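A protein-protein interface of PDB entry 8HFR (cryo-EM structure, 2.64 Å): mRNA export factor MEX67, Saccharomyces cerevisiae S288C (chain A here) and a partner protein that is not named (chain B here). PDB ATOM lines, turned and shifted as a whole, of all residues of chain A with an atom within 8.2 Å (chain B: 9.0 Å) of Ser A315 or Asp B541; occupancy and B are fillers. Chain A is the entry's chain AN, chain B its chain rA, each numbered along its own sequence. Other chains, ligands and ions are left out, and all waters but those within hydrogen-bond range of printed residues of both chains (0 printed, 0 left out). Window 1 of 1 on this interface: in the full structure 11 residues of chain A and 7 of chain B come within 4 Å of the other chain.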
ATOM      1  N   SER A 312      19.019 -17.827  12.440  1.00  0.00           N
ATOM      2  CA  SER A 312      19.854 -16.651  12.267  1.00  0.00           C
ATOM      3  C   SER A 312      19.822 -16.215  10.813  1.00  0.00           C
ATOM      4  O   SER A 312      19.621 -17.029   9.908  1.00  0.00           O
ATOM      5  CB  SER A 312      21.301 -16.911  12.692  1.00  0.00           C
ATOM      6  N   VAL A 313      20.034 -14.922  10.594  1.00  0.00           N
ATOM      7  CA  VAL A 313      20.156 -14.372   9.255  1.00  0.00           C
ATOM      8  C   VAL A 313      21.467 -13.613   9.155  1.00  0.00           C
ATOM      9  O   VAL A 313      21.781 -12.799  10.028  1.00  0.00           O
ATOM     10  CB  VAL A 313      18.978 -13.452   8.922  1.00  0.00           C
ATOM     11  N   ASP A 314      22.238 -13.891   8.107  1.00  0.00           N
ATOM     12  CA  ASP A 314      23.466 -13.150   7.812  1.00  0.00           C
ATOM     13  C   ASP A 314      23.141 -12.193   6.670  1.00  0.00           C
ATOM     14  O   ASP A 314      23.348 -12.508   5.497  1.00  0.00           O
ATOM     15  CB  ASP A 314      24.619 -14.083   7.456  1.00  0.00           C
ATOM     16  N   SER A 315      22.638 -11.009   7.023  1.00  0.00           N
ATOM     17  CA  SER A 315      22.090 -10.090   6.033  1.00  0.00           C
ATOM     18  C   SER A 315      23.155  -9.340   5.238  1.00  0.00           C
ATOM     19  O   SER A 315      22.791  -8.590   4.327  1.00  0.00           O
ATOM     20  CB  SER A 315      21.155  -9.092   6.717  1.00  0.00           C
ATOM     21  N   THR A 316      24.439  -9.524   5.548  1.00  0.00           N
ATOM     22  CA  THR A 316      25.502  -8.843   4.817  1.00  0.00           C
ATOM     23  C   THR A 316      25.617  -9.388   3.401  1.00  0.00           C
ATOM     24  O   THR A 316      25.620 -10.604   3.190  1.00  0.00           O
ATOM     25  CB  THR A 316      26.836  -9.002   5.548  1.00  0.00           C
ATOM     26  N   ILE A 317      25.704  -8.481   2.432  1.00  0.00           N
ATOM     27  CA  ILE A 317      25.772  -8.878   1.033  1.00  0.00           C
ATOM     28  C   ILE A 317      27.121  -9.508   0.727  1.00  0.00           C
ATOM     29  O   ILE A 317      28.157  -9.062   1.226  1.00  0.00           O
ATOM     30  CB  ILE A 317      25.535  -7.674   0.123  1.00  0.00           C
ATOM     31  N   PRO A 318      27.099 -10.555  -0.095  1.00  0.00           N
ATOM     32  CA  PRO A 318      28.296 -11.315  -0.419  1.00  0.00           C
ATOM     33  C   PRO A 318      29.263 -10.482  -1.259  1.00  0.00           C
ATOM     34  O   PRO A 318      28.912  -9.424  -1.791  1.00  0.00           O
ATOM     35  CB  PRO A 318      27.920 -12.596  -1.160  1.00  0.00           C
ATOM     36  N   ASP A 326      24.091 -13.367  -4.881  1.00  0.00           N
ATOM     37  CA  ASP A 326      22.855 -12.597  -4.806  1.00  0.00           C
ATOM     38  C   ASP A 326      23.172 -11.184  -4.329  1.00  0.00           C
ATOM     39  O   ASP A 326      23.659 -10.995  -3.209  1.00  0.00           O
ATOM     40  CB  ASP A 326      21.854 -13.276  -3.875  1.00  0.00           C
ATOM     41  N   GLN A 327      22.894 -10.195  -5.176  1.00  0.00           N
ATOM     42  CA  GLN A 327      23.312  -8.823  -4.922  1.00  0.00           C
ATOM     43  C   GLN A 327      22.256  -7.991  -4.211  1.00  0.00           C
ATOM     44  O   GLN A 327      22.595  -6.950  -3.638  1.00  0.00           O
ATOM     45  CB  GLN A 327      23.698  -8.139  -6.235  1.00  0.00           C
ATOM     46  N   THR A 328      20.995  -8.409  -4.233  1.00  0.00           N
ATOM     47  CA  THR A 328      19.923  -7.708  -3.521  1.00  0.00           C
ATOM     48  C   THR A 328      19.053  -8.779  -2.865  1.00  0.00           C
ATOM     49  O   THR A 328      18.092  -9.268  -3.464  1.00  0.00           O
ATOM     50  CB  THR A 328      19.127  -6.810  -4.457  1.00  0.00           C
ATOM     51  N   PRO A 329      19.392  -9.133  -1.632  1.00  0.00           N
ATOM     52  CA  PRO A 329      18.777 -10.265  -0.965  1.00  0.00           C
ATOM     53  C   PRO A 329      17.544  -9.842  -0.171  1.00  0.00           C
ATOM     54  O   PRO A 329      17.390  -8.685   0.223  1.00  0.00           O
ATOM     55  CB  PRO A 329      19.788 -10.955  -0.050  1.00  0.00           C
ATOM     56  N   ALA A 330      16.668 -10.815   0.072  1.00  0.00           N
ATOM     57  CA  ALA A 330      15.370 -10.598   0.699  1.00  0.00           C
ATOM     58  C   ALA A 330      15.217 -11.548   1.875  1.00  0.00           C
ATOM     59  O   ALA A 330      15.221 -12.768   1.691  1.00  0.00           O
ATOM     60  CB  ALA A 330      14.242 -10.820  -0.307  1.00  0.00           C
ATOM     61  N   PHE A 331      15.064 -10.992   3.077  1.00  0.00           N
ATOM     62  CA  PHE A 331      14.933 -11.809   4.276  1.00  0.00           C
ATOM     63  C   PHE A 331      13.839 -11.281   5.199  1.00  0.00           C
ATOM     64  O   PHE A 331      14.003 -11.287   6.426  1.00  0.00           O
ATOM     65  CB  PHE A 331      16.260 -11.890   5.028  1.00  0.00           C
ATOM     66  N   MET A 335      13.585 -12.493   9.067  1.00  0.00           N
ATOM     67  CA  MET A 335      14.022 -11.529  10.084  1.00  0.00           C
ATOM     68  C   MET A 335      13.001 -11.312  11.225  1.00  0.00           C
ATOM     69  O   MET A 335      13.187 -10.354  11.991  1.00  0.00           O
ATOM     70  CB  MET A 335      14.347 -10.188   9.425  1.00  0.00           C
ATOM     71  N   ASN A 340      20.089 -13.436  16.545  1.00  0.00           N
ATOM     72  CA  ASN A 340      21.417 -12.963  16.179  1.00  0.00           C
ATOM     73  C   ASN A 340      22.013 -12.212  17.358  1.00  0.00           C
ATOM     74  O   ASN A 340      21.503 -11.157  17.746  1.00  0.00           O
ATOM     75  CB  ASN A 340      21.350 -12.068  14.942  1.00  0.00           C
ATOM     76  N   LYS A 343      23.660  -8.902  15.999  1.00  0.00           N
ATOM     77  CA  LYS A 343      22.825  -7.992  15.233  1.00  0.00           C
ATOM     78  C   LYS A 343      21.561  -7.553  15.952  1.00  0.00           C
ATOM     79  O   LYS A 343      20.965  -6.551  15.549  1.00  0.00           O
ATOM     80  CB  LYS A 343      22.434  -8.621  13.887  1.00  0.00           C
ATOM     81  N   ASN A 433      11.083  -0.942   1.804  1.00  0.00           N
ATOM     82  CA  ASN A 433      12.416  -0.502   2.224  1.00  0.00           C
ATOM     83  C   ASN A 433      12.939  -0.954   3.590  1.00  0.00           C
ATOM     84  O   ASN A 433      14.132  -1.255   3.723  1.00  0.00           O
ATOM     85  CB  ASN A 433      12.447   1.026   2.186  1.00  0.00           C
ATOM     86  N   SER A 434      12.076  -0.999   4.613  1.00  0.00           N
ATOM     87  CA  SER A 434      12.513  -1.473   5.926  1.00  0.00           C
ATOM     88  C   SER A 434      12.698  -2.985   5.972  1.00  0.00           C
ATOM     89  O   SER A 434      13.377  -3.487   6.873  1.00  0.00           O
ATOM     90  CB  SER A 434      11.523  -1.047   7.008  1.00  0.00           C
ATOM     91  N   SER A 436      13.495  -4.786   2.838  1.00  0.00           N
ATOM     92  CA  SER A 436      13.604  -4.222   1.486  1.00  0.00           C
ATOM     93  C   SER A 436      12.976  -5.019   0.345  1.00  0.00           C
ATOM     94  O   SER A 436      12.481  -4.432  -0.622  1.00  0.00           O
ATOM     95  CB  SER A 436      15.083  -3.976   1.170  1.00  0.00           C
ATOM     96  N   VAL A 467      20.563 -18.677   7.702  1.00  0.00           N
ATOM     97  CA  VAL A 467      20.261 -18.365   6.313  1.00  0.00           C
ATOM     98  C   VAL A 467      21.107 -17.183   5.852  1.00  0.00           C
ATOM     99  O   VAL A 467      21.227 -16.181   6.565  1.00  0.00           O
ATOM    100  CB  VAL A 467      18.772 -18.062   6.135  1.00  0.00           C
ATOM    101  N   ARG A 468      21.680 -17.306   4.658  1.00  0.00           N
ATOM    102  CA  ARG A 468      22.555 -16.291   4.100  1.00  0.00           C
ATOM    103  C   ARG A 468      22.193 -16.059   2.641  1.00  0.00           C
ATOM    104  O   ARG A 468      21.433 -16.820   2.031  1.00  0.00           O
ATOM    105  CB  ARG A 468      24.028 -16.688   4.230  1.00  0.00           C
ATOM    106  N   ALA A 469      22.760 -14.988   2.086  1.00  0.00           N
ATOM    107  CA  ALA A 469      22.569 -14.664   0.681  1.00  0.00           C
ATOM    108  C   ALA A 469      23.241 -15.709  -0.196  1.00  0.00           C
ATOM    109  O   ALA A 469      24.240 -16.318   0.195  1.00  0.00           O
ATOM    110  CB  ALA A 469      23.130 -13.275   0.382  1.00  0.00           C
ATOM    111  N   GLU B 532      16.628   5.956   6.615  1.00  0.00           N
ATOM    112  CA  GLU B 532      16.429   4.572   6.212  1.00  0.00           C
ATOM    113  C   GLU B 532      15.939   4.494   4.777  1.00  0.00           C
ATOM    114  O   GLU B 532      16.311   3.574   4.038  1.00  0.00           O
ATOM    115  CB  GLU B 532      15.450   3.903   7.175  1.00  0.00           C
ATOM    116  CG  GLU B 532      15.551   2.394   7.244  1.00  0.00           C
ATOM    117  CD  GLU B 532      14.706   1.687   6.214  1.00  0.00           C
ATOM    118  OE1 GLU B 532      13.646   2.224   5.834  1.00  0.00           O
ATOM    119  OE2 GLU B 532      15.108   0.592   5.782  1.00  0.00           O
ATOM    120  N   MET B 535      19.169   5.115   2.671  1.00  0.00           N
ATOM    121  CA  MET B 535      20.070   3.967   2.679  1.00  0.00           C
ATOM    122  C   MET B 535      19.485   2.788   1.912  1.00  0.00           C
ATOM    123  O   MET B 535      20.223   2.035   1.265  1.00  0.00           O
ATOM    124  CB  MET B 535      20.396   3.557   4.112  1.00  0.00           C
ATOM    125  CG  MET B 535      21.247   4.542   4.866  1.00  0.00           C
ATOM    126  SD  MET B 535      22.549   5.257   3.868  1.00  0.00           S
ATOM    127  CE  MET B 535      23.321   6.332   5.066  1.00  0.00           C
ATOM    128  N   SER B 536      18.161   2.614   1.958  1.00  0.00           N
ATOM    129  CA  SER B 536      17.543   1.548   1.183  1.00  0.00           C
ATOM    130  C   SER B 536      17.586   1.854  -0.308  1.00  0.00           C
ATOM    131  O   SER B 536      17.684   0.937  -1.129  1.00  0.00           O
ATOM    132  CB  SER B 536      16.107   1.340   1.639  1.00  0.00           C
ATOM    133  OG  SER B 536      15.241   2.201   0.929  1.00  0.00           O
ATOM    134  N   THR B 537      17.509   3.134  -0.680  1.00  0.00           N
ATOM    135  CA  THR B 537      17.676   3.492  -2.085  1.00  0.00           C
ATOM    136  C   THR B 537      19.117   3.291  -2.537  1.00  0.00           C
ATOM    137  O   THR B 537      19.375   2.978  -3.704  1.00  0.00           O
ATOM    138  CB  THR B 537      17.233   4.938  -2.309  1.00  0.00           C
ATOM    139  OG1 THR B 537      16.016   5.177  -1.593  1.00  0.00           O
ATOM    140  CG2 THR B 537      16.990   5.212  -3.779  1.00  0.00           C
ATOM    141  N   LEU B 538      20.075   3.462  -1.624  1.00  0.00           N
ATOM    142  CA  LEU B 538      21.470   3.205  -1.971  1.00  0.00           C
ATOM    143  C   LEU B 538      21.732   1.718  -2.156  1.00  0.00           C
ATOM    144  O   LEU B 538      22.430   1.316  -3.090  1.00  0.00           O
ATOM    145  CB  LEU B 538      22.395   3.767  -0.898  1.00  0.00           C
ATOM    146  CG  LEU B 538      22.552   5.276  -0.897  1.00  0.00           C
ATOM    147  CD1 LEU B 538      23.381   5.692   0.289  1.00  0.00           C
ATOM    148  CD2 LEU B 538      23.187   5.714  -2.192  1.00  0.00           C
ATOM    149  N   GLY B 539      21.196   0.886  -1.271  1.00  0.00           N
ATOM    150  CA  GLY B 539      21.350  -0.543  -1.440  1.00  0.00           C
ATOM    151  C   GLY B 539      22.192  -1.209  -0.377  1.00  0.00           C
ATOM    152  O   GLY B 539      22.912  -2.169  -0.658  1.00  0.00           O
ATOM    153  N   HIS B 540      22.124  -0.701   0.842  1.00  0.00           N
ATOM    154  CA  HIS B 540      22.754  -1.340   1.983  1.00  0.00           C
ATOM    155  C   HIS B 540      21.706  -2.097   2.783  1.00  0.00           C
ATOM    156  O   HIS B 540      20.511  -2.054   2.489  1.00  0.00           O
ATOM    157  CB  HIS B 540      23.460  -0.304   2.859  1.00  0.00           C
ATOM    158  CG  HIS B 540      24.335   0.637   2.093  1.00  0.00           C
ATOM    159  ND1 HIS B 540      25.571   0.274   1.604  1.00  0.00           N
ATOM    160  CD2 HIS B 540      24.151   1.927   1.731  1.00  0.00           C
ATOM    161  CE1 HIS B 540      26.110   1.302   0.975  1.00  0.00           C
ATOM    162  NE2 HIS B 540      25.269   2.316   1.037  1.00  0.00           N
ATOM    163  N   ASP B 541      22.167  -2.812   3.805  1.00  0.00           N
ATOM    164  CA  ASP B 541      21.285  -3.460   4.764  1.00  0.00           C
ATOM    165  C   ASP B 541      21.271  -2.671   6.063  1.00  0.00           C
ATOM    166  O   ASP B 541      22.324  -2.270   6.568  1.00  0.00           O
ATOM    167  CB  ASP B 541      21.697  -4.911   5.013  1.00  0.00           C
ATOM    168  CG  ASP B 541      23.169  -5.062   5.272  1.00  0.00           C
ATOM    169  OD1 ASP B 541      23.913  -4.092   5.037  1.00  0.00           O
ATOM    170  OD2 ASP B 541      23.583  -6.144   5.724  1.00  0.00           O
ATOM    171  N   MET B 542      20.075  -2.432   6.589  1.00  0.00           N
ATOM    172  CA  MET B 542      19.894  -1.584   7.764  1.00  0.00           C
ATOM    173  C   MET B 542      19.652  -2.391   9.027  1.00  0.00           C
ATOM    174  O   MET B 542      18.890  -1.964   9.891  1.00  0.00           O
ATOM    175  CB  MET B 542      18.751  -0.601   7.537  1.00  0.00           C
ATOM    176  CG  MET B 542      19.141   0.611   6.724  1.00  0.00           C
ATOM    177  SD  MET B 542      19.578   0.144   5.053  1.00  0.00           S
ATOM    178  CE  MET B 542      17.992  -0.418   4.454  1.00  0.00           C
ATOM    179  N   SER B 543      20.302  -3.544   9.171  1.00  0.00           N
ATOM    180  CA  SER B 543      20.118  -4.347  10.376  1.00  0.00           C
ATOM    181  C   SER B 543      20.778  -3.694  11.588  1.00  0.00           C
ATOM    182  O   SER B 543      20.154  -3.560  12.649  1.00  0.00           O
ATOM    183  CB  SER B 543      20.659  -5.757  10.143  1.00  0.00           C
ATOM    184  OG  SER B 543      21.889  -5.712   9.453  1.00  0.00           O
ATOM    185  N   ALA B 544      22.027  -3.238  11.433  1.00  0.00           N
ATOM    186  CA  ALA B 544      22.729  -2.575  12.528  1.00  0.00           C
ATOM    187  C   ALA B 544      22.112  -1.218  12.853  1.00  0.00           C
ATOM    188  O   ALA B 544      21.983  -0.852  14.029  1.00  0.00           O
ATOM    189  CB  ALA B 544      24.207  -2.427  12.177  1.00  0.00           C
ATOM    190  N   LEU B 545      21.691  -0.477  11.825  1.00  0.00           N
ATOM    191  CA  LEU B 545      21.043   0.812  12.039  1.00  0.00           C
ATOM    192  C   LEU B 545      19.677   0.652  12.698  1.00  0.00           C
ATOM    193  O   LEU B 545      19.308   1.442  13.578  1.00  0.00           O
ATOM    194  CB  LEU B 545      20.921   1.549  10.707  1.00  0.00           C
ATOM    195  CG  LEU B 545      21.951   2.629  10.382  1.00  0.00           C
ATOM    196  CD1 LEU B 545      23.359   2.109  10.431  1.00  0.00           C
ATOM    197  CD2 LEU B 545      21.666   3.175   9.001  1.00  0.00           C
ATOM    198  N   GLN B 546      18.929  -0.381  12.309  1.00  0.00           N
ATOM    199  CA  GLN B 546      17.638  -0.642  12.931  1.00  0.00           C
ATOM    200  C   GLN B 546      17.806  -1.097  14.379  1.00  0.00           C
ATOM    201  O   GLN B 546      16.985  -0.765  15.242  1.00  0.00           O
ATOM    202  CB  GLN B 546      16.882  -1.682  12.111  1.00  0.00           C
ATOM    203  CG  GLN B 546      15.419  -1.802  12.444  1.00  0.00           C
ATOM    204  CD  GLN B 546      14.671  -0.512  12.234  1.00  0.00           C
ATOM    205  OE1 GLN B 546      14.404   0.221  13.182  1.00  0.00           O
ATOM    206  NE2 GLN B 546      14.320  -0.228  10.988  1.00  0.00           N
ATOM    207  N   ASP B 547      18.898  -1.810  14.669  1.00  0.00           N
ATOM    208  CA  ASP B 547      19.214  -2.183  16.045  1.00  0.00           C
ATOM    209  C   ASP B 547      19.526  -0.966  16.912  1.00  0.00           C
ATOM    210  O   ASP B 547      19.050  -0.870  18.054  1.00  0.00           O
ATOM    211  CB  ASP B 547      20.390  -3.151  16.051  1.00  0.00           C
ATOM    212  CG  ASP B 547      20.484  -3.943  17.329  1.00  0.00           C
ATOM    213  OD1 ASP B 547      19.445  -4.469  17.777  1.00  0.00           O
ATOM    214  OD2 ASP B 547      21.601  -4.048  17.882  1.00  0.00           O
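Among the printed residues, pairs that only touch across the chains: Asn A433 with Ser B536 (3.3 Å) and Ser A434 with Glu B532 (3.3 Å).
The backbone carbonyl oxygen (O) of Lys A343 lies close to the side-chain carboxylate (OD1) of Asp B547, 3.4 Å away. The side-chain carboxylate (OE2) of Glu B532 lies close to the backbone carbonyl oxygen (O) of Asn A433 (2.9 Å). The backbone carbonyl oxygen (O) of Ser A315 sits close to the side-chain carboxylate (OD2) of Asp B541, 2.9 Å away. The backbone NH (N) of Thr A316 sits close to the side-chain carboxylate (OD2) of Asp B541 (3.5 Å).
Of chain B, only Asp B541 (2.9 Å) comes within 4 Å of Ser A315. Printed residues of chain A within 4 Å of Asp B541: Ser A315 (2.9 Å) and Thr A316 (3.4 Å). No residue of chain B comes within 4 Å of Asp A314. Thr A316 touches just one residue of chain B: Asp B541 (3.4 Å). Of the printed residues of chain B, Asn A433 touches Glu B532 and Ser B536. Printed residues of chain A within 4 Å of Asp B547: Lys A343 (3.2 Å). Printed residues of chain B within 4 Å of Lys A343: Asp B547 (3.2 Å). The nearest residue of chain B that does not touch Ser A315 is Ser B543 (4.4 Å). The nearest residue of chain A that does not touch Asp B541 is Ile A317 (4.6 Å). The nearest printed residue of chain B that does not touch Asn A433 is Met B542 (4.02 Å).
Among the printed residues, 6 pairs touch across the chains. Among the printed residues, no Asp or Glu carboxylate lies within 4 Å of a Lys or Arg side-chain nitrogen of the other chain.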
